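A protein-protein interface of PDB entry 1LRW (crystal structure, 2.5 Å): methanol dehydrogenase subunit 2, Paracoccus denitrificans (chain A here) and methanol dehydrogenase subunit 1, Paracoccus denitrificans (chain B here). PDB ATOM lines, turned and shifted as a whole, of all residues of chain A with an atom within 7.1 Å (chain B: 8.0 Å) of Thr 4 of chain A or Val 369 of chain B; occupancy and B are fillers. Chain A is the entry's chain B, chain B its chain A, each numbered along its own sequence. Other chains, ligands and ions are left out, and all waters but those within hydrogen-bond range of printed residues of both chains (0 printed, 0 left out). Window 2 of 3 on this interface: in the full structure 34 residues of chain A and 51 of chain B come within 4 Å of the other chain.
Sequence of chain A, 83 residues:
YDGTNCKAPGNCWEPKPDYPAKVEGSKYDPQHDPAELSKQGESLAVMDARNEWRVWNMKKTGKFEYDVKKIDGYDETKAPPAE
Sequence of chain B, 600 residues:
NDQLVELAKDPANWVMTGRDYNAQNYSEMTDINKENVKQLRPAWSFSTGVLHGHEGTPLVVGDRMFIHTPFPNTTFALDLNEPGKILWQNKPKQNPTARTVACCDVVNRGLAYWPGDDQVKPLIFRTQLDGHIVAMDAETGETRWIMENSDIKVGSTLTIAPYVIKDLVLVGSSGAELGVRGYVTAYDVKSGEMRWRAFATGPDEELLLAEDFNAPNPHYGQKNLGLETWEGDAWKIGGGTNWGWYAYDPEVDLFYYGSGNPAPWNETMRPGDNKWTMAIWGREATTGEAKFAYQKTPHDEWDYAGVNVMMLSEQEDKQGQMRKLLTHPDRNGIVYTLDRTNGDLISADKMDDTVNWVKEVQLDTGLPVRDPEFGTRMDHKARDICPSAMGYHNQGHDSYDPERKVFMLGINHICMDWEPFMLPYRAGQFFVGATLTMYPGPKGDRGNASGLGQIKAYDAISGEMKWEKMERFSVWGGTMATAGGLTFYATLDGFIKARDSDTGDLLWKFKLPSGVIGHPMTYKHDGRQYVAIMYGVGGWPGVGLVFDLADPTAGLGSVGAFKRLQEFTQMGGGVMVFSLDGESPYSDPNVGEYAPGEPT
OH of Tyr 1 of chain A is in hydrogen-bond range of NH2 of Arg 370 of chain B, 3.5 Å away.
The backbone carbonyl oxygen (O) of Asp 2 of chain A lies within hydrogen-bond range of the backbone NH (N) of Arg 370 of chain B.
The backbone NH (N) of Lys 359 of chain B is in hydrogen-bond range of the backbone carbonyl oxygen (O) of Val 369 of chain B (3.0 Å).
O of Glu 360 of chain B is in hydrogen-bond range of N of Val 369 of chain B, 2.9 Å away.
The backbone carbonyl oxygen (O) of Leu 367 of chain B is in hydrogen-bond range of the backbone NH (N) of Gln 362 of chain B (3.2 Å).
The side-chain hydroxyl (OG1) of Thr 365 of chain B is in hydrogen-bond range of the backbone NH (N) of Leu 367 of chain B (3.1 Å).
The side-chain hydroxyl (OG1) of Thr 4 of chain A lies within hydrogen-bond range of the side-chain carboxylate (OD2) of Asp 2 of chain A, at 2.6 Å.
The side-chain sulfur (SG) of Cys 12 of chain A is disulfide-bonded to the side-chain sulfur (SG) of Cys 6 of chain A (2.0 Å).
Tyr 1 of chain A touches Pro 372 of chain B.
Asp 2 of chain A touches Pro 368 of chain B (O to O, 3.5 Å).
CA of Val 369 of chain B touches O of Asp 2 of chain A, 3.6 Å away.
O of Gly 3 of chain A touches CD2 of Leu 367 of chain B, 3.3 Å away.
CG2 of Val 369 of chain B touches CG2 of Thr 4 of chain A, at 3.998 Å.
SG of Cys 6 of chain A touches CD2 of Leu 367 of chain B, 3.4 Å away.
CD2 of Leu 367 of chain B touches SG of Cys 12 of chain A, 3.8 Å away.
Of the printed residues of chain B, Tyr 1 of chain A touches Arg 370 and Pro 372.
Of chain B, only Leu 367 comes within 4 Å of Gly 3 of chain A.
Of the printed residues of chain B, Thr 4 of chain A touches Val 369 (3.998 Å).
Glu 14 of chain A touches none of the printed residues of chain B.
Val 361 of chain B touches none of the printed residues of chain A.
Of the printed residues of chain A, Val 369 of chain B touches Asp 2 and Thr 4.
Of the printed residues of chain A, Pro 372 of chain B touches Tyr 1 (3.9 Å).
The nearest printed residue of chain B that does not touch Thr 4 of chain A is Leu 367 of chain B (4.01 Å).
Of the 8 printed residues of chain A, 6 touch a printed residue of chain B.
Printed residues of chain A that touch a printed residue of chain B: Tyr 1, Asp 2, Gly 3, Thr 4, Cys 6 and Cys 12.
Hydrophobic or aromatic side chains of chain A within 4 Å of the printed part of chain B: Tyr 1.
Of the 16 printed residues of chain B, 5 touch a printed residue of chain A.
Hydrophobic or aromatic side chains of chain B within 4 Å of the printed part of chain A: Leu 367, Val 369 and Pro 372.
Among the printed residues, 9 pairs touch across the chains.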
ATOM      1  N   TYR A   1     -21.587 -19.203  -9.171  1.00  0.00           N
ATOM      2  CA  TYR A   1     -23.021 -19.322  -8.779  1.00  0.00           C
ATOM      3  C   TYR A   1     -23.183 -20.298  -7.625  1.00  0.00           C
ATOM      4  O   TYR A   1     -23.323 -21.502  -7.838  1.00  0.00           O
ATOM      5  CB  TYR A   1     -23.845 -19.795  -9.975  1.00  0.00           C
ATOM      6  CG  TYR A   1     -25.295 -20.088  -9.661  1.00  0.00           C
ATOM      7  CD1 TYR A   1     -26.058 -19.204  -8.902  1.00  0.00           C
ATOM      8  CD2 TYR A   1     -25.915 -21.236 -10.155  1.00  0.00           C
ATOM      9  CE1 TYR A   1     -27.406 -19.454  -8.644  1.00  0.00           C
ATOM     10  CE2 TYR A   1     -27.264 -21.492  -9.903  1.00  0.00           C
ATOM     11  CZ  TYR A   1     -28.000 -20.596  -9.149  1.00  0.00           C
ATOM     12  OH  TYR A   1     -29.328 -20.832  -8.906  1.00  0.00           O
ATOM     13  N   ASP A   2     -23.159 -19.770  -6.405  1.00  0.00           N
ATOM     14  CA  ASP A   2     -23.298 -20.588  -5.208  1.00  0.00           C
ATOM     15  C   ASP A   2     -24.684 -20.455  -4.602  1.00  0.00           C
ATOM     16  O   ASP A   2     -24.996 -21.110  -3.609  1.00  0.00           O
ATOM     17  CB  ASP A   2     -22.237 -20.201  -4.172  1.00  0.00           C
ATOM     18  CG  ASP A   2     -22.365 -18.761  -3.697  1.00  0.00           C
ATOM     19  OD1 ASP A   2     -21.495 -18.326  -2.919  1.00  0.00           O
ATOM     20  OD2 ASP A   2     -23.323 -18.063  -4.087  1.00  0.00           O
ATOM     21  N   GLY A   3     -25.504 -19.596  -5.204  1.00  0.00           N
ATOM     22  CA  GLY A   3     -26.865 -19.387  -4.737  1.00  0.00           C
ATOM     23  C   GLY A   3     -27.052 -18.413  -3.588  1.00  0.00           C
ATOM     24  O   GLY A   3     -28.152 -18.323  -3.032  1.00  0.00           O
ATOM     25  N   THR A   4     -26.005 -17.671  -3.234  1.00  0.00           N
ATOM     26  CA  THR A   4     -26.096 -16.726  -2.124  1.00  0.00           C
ATOM     27  C   THR A   4     -26.055 -15.250  -2.487  1.00  0.00           C
ATOM     28  O   THR A   4     -26.227 -14.399  -1.614  1.00  0.00           O
ATOM     29  CB  THR A   4     -24.993 -16.984  -1.088  1.00  0.00           C
ATOM     30  OG1 THR A   4     -23.729 -17.084  -1.755  1.00  0.00           O
ATOM     31  CG2 THR A   4     -25.280 -18.265  -0.316  1.00  0.00           C
ATOM     32  N   ASN A   5     -25.817 -14.943  -3.758  1.00  0.00           N
ATOM     33  CA  ASN A   5     -25.774 -13.554  -4.207  1.00  0.00           C
ATOM     34  C   ASN A   5     -27.098 -13.223  -4.890  1.00  0.00           C
ATOM     35  O   ASN A   5     -27.265 -13.443  -6.088  1.00  0.00           O
ATOM     36  CB  ASN A   5     -24.616 -13.338  -5.181  1.00  0.00           C
ATOM     37  CG  ASN A   5     -24.369 -11.865  -5.465  1.00  0.00           C
ATOM     38  OD1 ASN A   5     -25.274 -11.138  -5.890  1.00  0.00           O
ATOM     39  ND2 ASN A   5     -23.141 -11.414  -5.223  1.00  0.00           N
ATOM     40  N   CYS A   6     -28.028 -12.671  -4.124  1.00  0.00           N
ATOM     41  CA  CYS A   6     -29.355 -12.358  -4.634  1.00  0.00           C
ATOM     42  C   CYS A   6     -29.549 -10.946  -5.197  1.00  0.00           C
ATOM     43  O   CYS A   6     -29.120  -9.970  -4.588  1.00  0.00           O
ATOM     44  CB  CYS A   6     -30.370 -12.613  -3.514  1.00  0.00           C
ATOM     45  SG  CYS A   6     -30.134 -14.213  -2.657  1.00  0.00           S
ATOM     46  N   CYS A  12     -32.009 -15.238  -6.561  1.00  0.00           N
ATOM     47  CA  CYS A  12     -30.568 -15.371  -6.376  1.00  0.00           C
ATOM     48  C   CYS A  12     -29.818 -16.064  -7.512  1.00  0.00           C
ATOM     49  O   CYS A  12     -28.651 -16.427  -7.357  1.00  0.00           O
ATOM     50  CB  CYS A  12     -30.302 -16.101  -5.054  1.00  0.00           C
ATOM     51  SG  CYS A  12     -31.341 -15.488  -3.681  1.00  0.00           S
ATOM     52  N   GLU A  14     -27.684 -16.713 -10.883  1.00  0.00           N
ATOM     53  CA  GLU A  14     -26.548 -16.079 -11.542  1.00  0.00           C
ATOM     54  C   GLU A  14     -26.086 -17.067 -12.595  1.00  0.00           C
ATOM     55  O   GLU A  14     -26.149 -18.276 -12.388  1.00  0.00           O
ATOM     56  CB  GLU A  14     -25.386 -15.859 -10.574  1.00  0.00           C
ATOM     57  CG  GLU A  14     -25.653 -14.945  -9.409  1.00  0.00           C
ATOM     58  CD  GLU A  14     -24.447 -14.847  -8.503  1.00  0.00           C
ATOM     59  OE1 GLU A  14     -24.069 -15.879  -7.903  1.00  0.00           O
ATOM     60  OE2 GLU A  14     -23.872 -13.740  -8.400  1.00  0.00           O
ATOM     61  N   LYS B 350     -29.229 -32.966   6.340  1.00  0.00           N
ATOM     62  CA  LYS B 350     -28.976 -33.901   5.250  1.00  0.00           C
ATOM     63  C   LYS B 350     -29.343 -35.271   5.797  1.00  0.00           C
ATOM     64  O   LYS B 350     -28.907 -35.622   6.891  1.00  0.00           O
ATOM     65  CB  LYS B 350     -27.496 -33.912   4.876  1.00  0.00           C
ATOM     66  CG  LYS B 350     -26.951 -32.605   4.349  1.00  0.00           C
ATOM     67  CD  LYS B 350     -25.535 -32.811   3.854  1.00  0.00           C
ATOM     68  CE  LYS B 350     -25.050 -31.644   3.020  1.00  0.00           C
ATOM     69  NZ  LYS B 350     -23.653 -31.849   2.526  1.00  0.00           N
ATOM     70  N   ASN B 356     -24.052 -34.283  -1.823  1.00  0.00           N
ATOM     71  CA  ASN B 356     -23.020 -33.316  -2.167  1.00  0.00           C
ATOM     72  C   ASN B 356     -23.386 -32.154  -3.084  1.00  0.00           C
ATOM     73  O   ASN B 356     -22.530 -31.320  -3.371  1.00  0.00           O
ATOM     74  CB  ASN B 356     -21.808 -34.041  -2.750  1.00  0.00           C
ATOM     75  CG  ASN B 356     -22.146 -34.812  -4.004  1.00  0.00           C
ATOM     76  OD1 ASN B 356     -23.073 -34.449  -4.731  1.00  0.00           O
ATOM     77  ND2 ASN B 356     -21.386 -35.872  -4.277  1.00  0.00           N
ATOM     78  N   TRP B 357     -24.626 -32.071  -3.556  1.00  0.00           N
ATOM     79  CA  TRP B 357     -24.968 -30.945  -4.427  1.00  0.00           C
ATOM     80  C   TRP B 357     -24.998 -29.655  -3.602  1.00  0.00           C
ATOM     81  O   TRP B 357     -24.844 -28.553  -4.139  1.00  0.00           O
ATOM     82  CB  TRP B 357     -26.321 -31.156  -5.122  1.00  0.00           C
ATOM     83  CG  TRP B 357     -27.502 -31.049  -4.215  1.00  0.00           C
ATOM     84  CD1 TRP B 357     -28.017 -32.029  -3.412  1.00  0.00           C
ATOM     85  CD2 TRP B 357     -28.291 -29.877  -3.976  1.00  0.00           C
ATOM     86  NE1 TRP B 357     -29.075 -31.537  -2.686  1.00  0.00           N
ATOM     87  CE2 TRP B 357     -29.266 -30.218  -3.012  1.00  0.00           C
ATOM     88  CE3 TRP B 357     -28.268 -28.572  -4.483  1.00  0.00           C
ATOM     89  CZ2 TRP B 357     -30.214 -29.297  -2.541  1.00  0.00           C
ATOM     90  CZ3 TRP B 357     -29.212 -27.654  -4.015  1.00  0.00           C
ATOM     91  CH2 TRP B 357     -30.171 -28.025  -3.051  1.00  0.00           C
ATOM     92  N   VAL B 358     -25.210 -29.806  -2.295  1.00  0.00           N
ATOM     93  CA  VAL B 358     -25.233 -28.678  -1.368  1.00  0.00           C
ATOM     94  C   VAL B 358     -24.244 -28.889  -0.244  1.00  0.00           C
ATOM     95  O   VAL B 358     -24.072 -30.007   0.259  1.00  0.00           O
ATOM     96  CB  VAL B 358     -26.600 -28.465  -0.680  1.00  0.00           C
ATOM     97  CG1 VAL B 358     -27.423 -27.482  -1.463  1.00  0.00           C
ATOM     98  CG2 VAL B 358     -27.321 -29.790  -0.505  1.00  0.00           C
ATOM     99  N   LYS B 359     -23.590 -27.804   0.150  1.00  0.00           N
ATOM    100  CA  LYS B 359     -22.653 -27.881   1.243  1.00  0.00           C
ATOM    101  C   LYS B 359     -23.502 -27.785   2.504  1.00  0.00           C
ATOM    102  O   LYS B 359     -23.303 -28.546   3.451  1.00  0.00           O
ATOM    103  CB  LYS B 359     -21.643 -26.736   1.159  1.00  0.00           C
ATOM    104  CG  LYS B 359     -20.785 -26.777  -0.099  1.00  0.00           C
ATOM    105  CD  LYS B 359     -19.608 -25.819   0.000  1.00  0.00           C
ATOM    106  CE  LYS B 359     -18.669 -25.963  -1.195  1.00  0.00           C
ATOM    107  NZ  LYS B 359     -17.386 -25.211  -1.018  1.00  0.00           N
ATOM    108  N   GLU B 360     -24.472 -26.873   2.498  1.00  0.00           N
ATOM    109  CA  GLU B 360     -25.359 -26.695   3.643  1.00  0.00           C
ATOM    110  C   GLU B 360     -26.486 -25.704   3.374  1.00  0.00           C
ATOM    111  O   GLU B 360     -26.437 -24.923   2.421  1.00  0.00           O
ATOM    112  CB  GLU B 360     -24.564 -26.210   4.856  1.00  0.00           C
ATOM    113  CG  GLU B 360     -23.888 -24.856   4.641  1.00  0.00           C
ATOM    114  CD  GLU B 360     -23.229 -24.315   5.902  1.00  0.00           C
ATOM    115  OE1 GLU B 360     -23.948 -24.093   6.905  1.00  0.00           O
ATOM    116  OE2 GLU B 360     -21.993 -24.112   5.888  1.00  0.00           O
ATOM    117  N   VAL B 361     -27.503 -25.745   4.228  1.00  0.00           N
ATOM    118  CA  VAL B 361     -28.643 -24.840   4.125  1.00  0.00           C
ATOM    119  C   VAL B 361     -28.579 -23.865   5.298  1.00  0.00           C
ATOM    120  O   VAL B 361     -28.522 -24.278   6.460  1.00  0.00           O
ATOM    121  CB  VAL B 361     -29.995 -25.604   4.187  1.00  0.00           C
ATOM    122  CG1 VAL B 361     -31.153 -24.619   4.155  1.00  0.00           C
ATOM    123  CG2 VAL B 361     -30.107 -26.568   3.025  1.00  0.00           C
ATOM    124  N   GLN B 362     -28.584 -22.572   4.998  1.00  0.00           N
ATOM    125  CA  GLN B 362     -28.523 -21.560   6.043  1.00  0.00           C
ATOM    126  C   GLN B 362     -29.926 -21.308   6.569  1.00  0.00           C
ATOM    127  O   GLN B 362     -30.810 -20.901   5.819  1.00  0.00           O
ATOM    128  CB  GLN B 362     -27.939 -20.272   5.485  1.00  0.00           C
ATOM    129  CG  GLN B 362     -26.878 -20.517   4.445  1.00  0.00           C
ATOM    130  CD  GLN B 362     -26.276 -19.241   3.932  1.00  0.00           C
ATOM    131  OE1 GLN B 362     -26.970 -18.237   3.775  1.00  0.00           O
ATOM    132  NE2 GLN B 362     -24.979 -19.271   3.650  1.00  0.00           N
ATOM    133  N   THR B 365     -31.090 -17.417   6.192  1.00  0.00           N
ATOM    134  CA  THR B 365     -31.447 -16.916   4.873  1.00  0.00           C
ATOM    135  C   THR B 365     -32.336 -17.931   4.180  1.00  0.00           C
ATOM    136  O   THR B 365     -33.202 -17.566   3.387  1.00  0.00           O
ATOM    137  CB  THR B 365     -30.206 -16.682   3.993  1.00  0.00           C
ATOM    138  OG1 THR B 365     -29.609 -17.940   3.659  1.00  0.00           O
ATOM    139  CG2 THR B 365     -29.192 -15.844   4.725  1.00  0.00           C
ATOM    140  N   GLY B 366     -32.116 -19.207   4.488  1.00  0.00           N
ATOM    141  CA  GLY B 366     -32.901 -20.270   3.886  1.00  0.00           C
ATOM    142  C   GLY B 366     -32.355 -20.679   2.530  1.00  0.00           C
ATOM    143  O   GLY B 366     -32.941 -21.506   1.831  1.00  0.00           O
ATOM    144  N   LEU B 367     -31.226 -20.094   2.155  1.00  0.00           N
ATOM    145  CA  LEU B 367     -30.607 -20.399   0.874  1.00  0.00           C
ATOM    146  C   LEU B 367     -29.674 -21.591   0.973  1.00  0.00           C
ATOM    147  O   LEU B 367     -28.938 -21.727   1.945  1.00  0.00           O
ATOM    148  CB  LEU B 367     -29.827 -19.187   0.363  1.00  0.00           C
ATOM    149  CG  LEU B 367     -30.637 -18.094  -0.334  1.00  0.00           C
ATOM    150  CD1 LEU B 367     -31.894 -17.767   0.454  1.00  0.00           C
ATOM    151  CD2 LEU B 367     -29.760 -16.870  -0.499  1.00  0.00           C
ATOM    152  N   PRO B 368     -29.704 -22.479  -0.034  1.00  0.00           N
ATOM    153  CA  PRO B 368     -28.838 -23.660  -0.035  1.00  0.00           C
ATOM    154  C   PRO B 368     -27.541 -23.266  -0.722  1.00  0.00           C
ATOM    155  O   PRO B 368     -27.576 -22.738  -1.831  1.00  0.00           O
ATOM    156  CB  PRO B 368     -29.626 -24.677  -0.869  1.00  0.00           C
ATOM    157  CG  PRO B 368     -30.997 -24.020  -1.099  1.00  0.00           C
ATOM    158  CD  PRO B 368     -30.689 -22.568  -1.119  1.00  0.00           C
ATOM    159  N   VAL B 369     -26.403 -23.501  -0.078  1.00  0.00           N
ATOM    160  CA  VAL B 369     -25.127 -23.143  -0.685  1.00  0.00           C
ATOM    161  C   VAL B 369     -24.687 -24.217  -1.672  1.00  0.00           C
ATOM    162  O   VAL B 369     -24.123 -25.241  -1.293  1.00  0.00           O
ATOM    163  CB  VAL B 369     -24.018 -22.944   0.382  1.00  0.00           C
ATOM    164  CG1 VAL B 369     -22.688 -22.646  -0.301  1.00  0.00           C
ATOM    165  CG2 VAL B 369     -24.389 -21.803   1.320  1.00  0.00           C
ATOM    166  N   ARG B 370     -24.952 -23.972  -2.946  1.00  0.00           N
ATOM    167  CA  ARG B 370     -24.593 -24.917  -3.992  1.00  0.00           C
ATOM    168  C   ARG B 370     -23.091 -25.137  -4.062  1.00  0.00           C
ATOM    169  O   ARG B 370     -22.313 -24.240  -3.763  1.00  0.00           O
ATOM    170  CB  ARG B 370     -25.044 -24.403  -5.356  1.00  0.00           C
ATOM    171  CG  ARG B 370     -26.461 -23.897  -5.425  1.00  0.00           C
ATOM    172  CD  ARG B 370     -26.659 -23.171  -6.743  1.00  0.00           C
ATOM    173  NE  ARG B 370     -27.380 -23.949  -7.745  1.00  0.00           N
ATOM    174  CZ  ARG B 370     -28.698 -24.116  -7.734  1.00  0.00           C
ATOM    175  NH1 ARG B 370     -29.291 -24.829  -8.684  1.00  0.00           N
ATOM    176  NH2 ARG B 370     -29.419 -23.565  -6.765  1.00  0.00           N
ATOM    177  N   ASP B 371     -22.700 -26.341  -4.462  1.00  0.00           N
ATOM    178  CA  ASP B 371     -21.297 -26.689  -4.642  1.00  0.00           C
ATOM    179  C   ASP B 371     -21.180 -26.815  -6.156  1.00  0.00           C
ATOM    180  O   ASP B 371     -21.511 -27.846  -6.737  1.00  0.00           O
ATOM    181  CB  ASP B 371     -20.965 -28.023  -3.962  1.00  0.00           C
ATOM    182  CG  ASP B 371     -19.544 -28.497  -4.258  1.00  0.00           C
ATOM    183  OD1 ASP B 371     -19.077 -29.440  -3.586  1.00  0.00           O
ATOM    184  OD2 ASP B 371     -18.893 -27.939  -5.165  1.00  0.00           O
ATOM    185  N   PRO B 372     -20.718 -25.748  -6.817  1.00  0.00           N
ATOM    186  CA  PRO B 372     -20.565 -25.729  -8.273  1.00  0.00           C
ATOM    187  C   PRO B 372     -20.058 -27.026  -8.898  1.00  0.00           C
ATOM    188  O   PRO B 372     -20.450 -27.383 -10.009  1.00  0.00           O
ATOM    189  CB  PRO B 372     -19.622 -24.552  -8.494  1.00  0.00           C
ATOM    190  CG  PRO B 372     -20.066 -23.591  -7.419  1.00  0.00           C
ATOM    191  CD  PRO B 372     -20.184 -24.511  -6.216  1.00  0.00           C
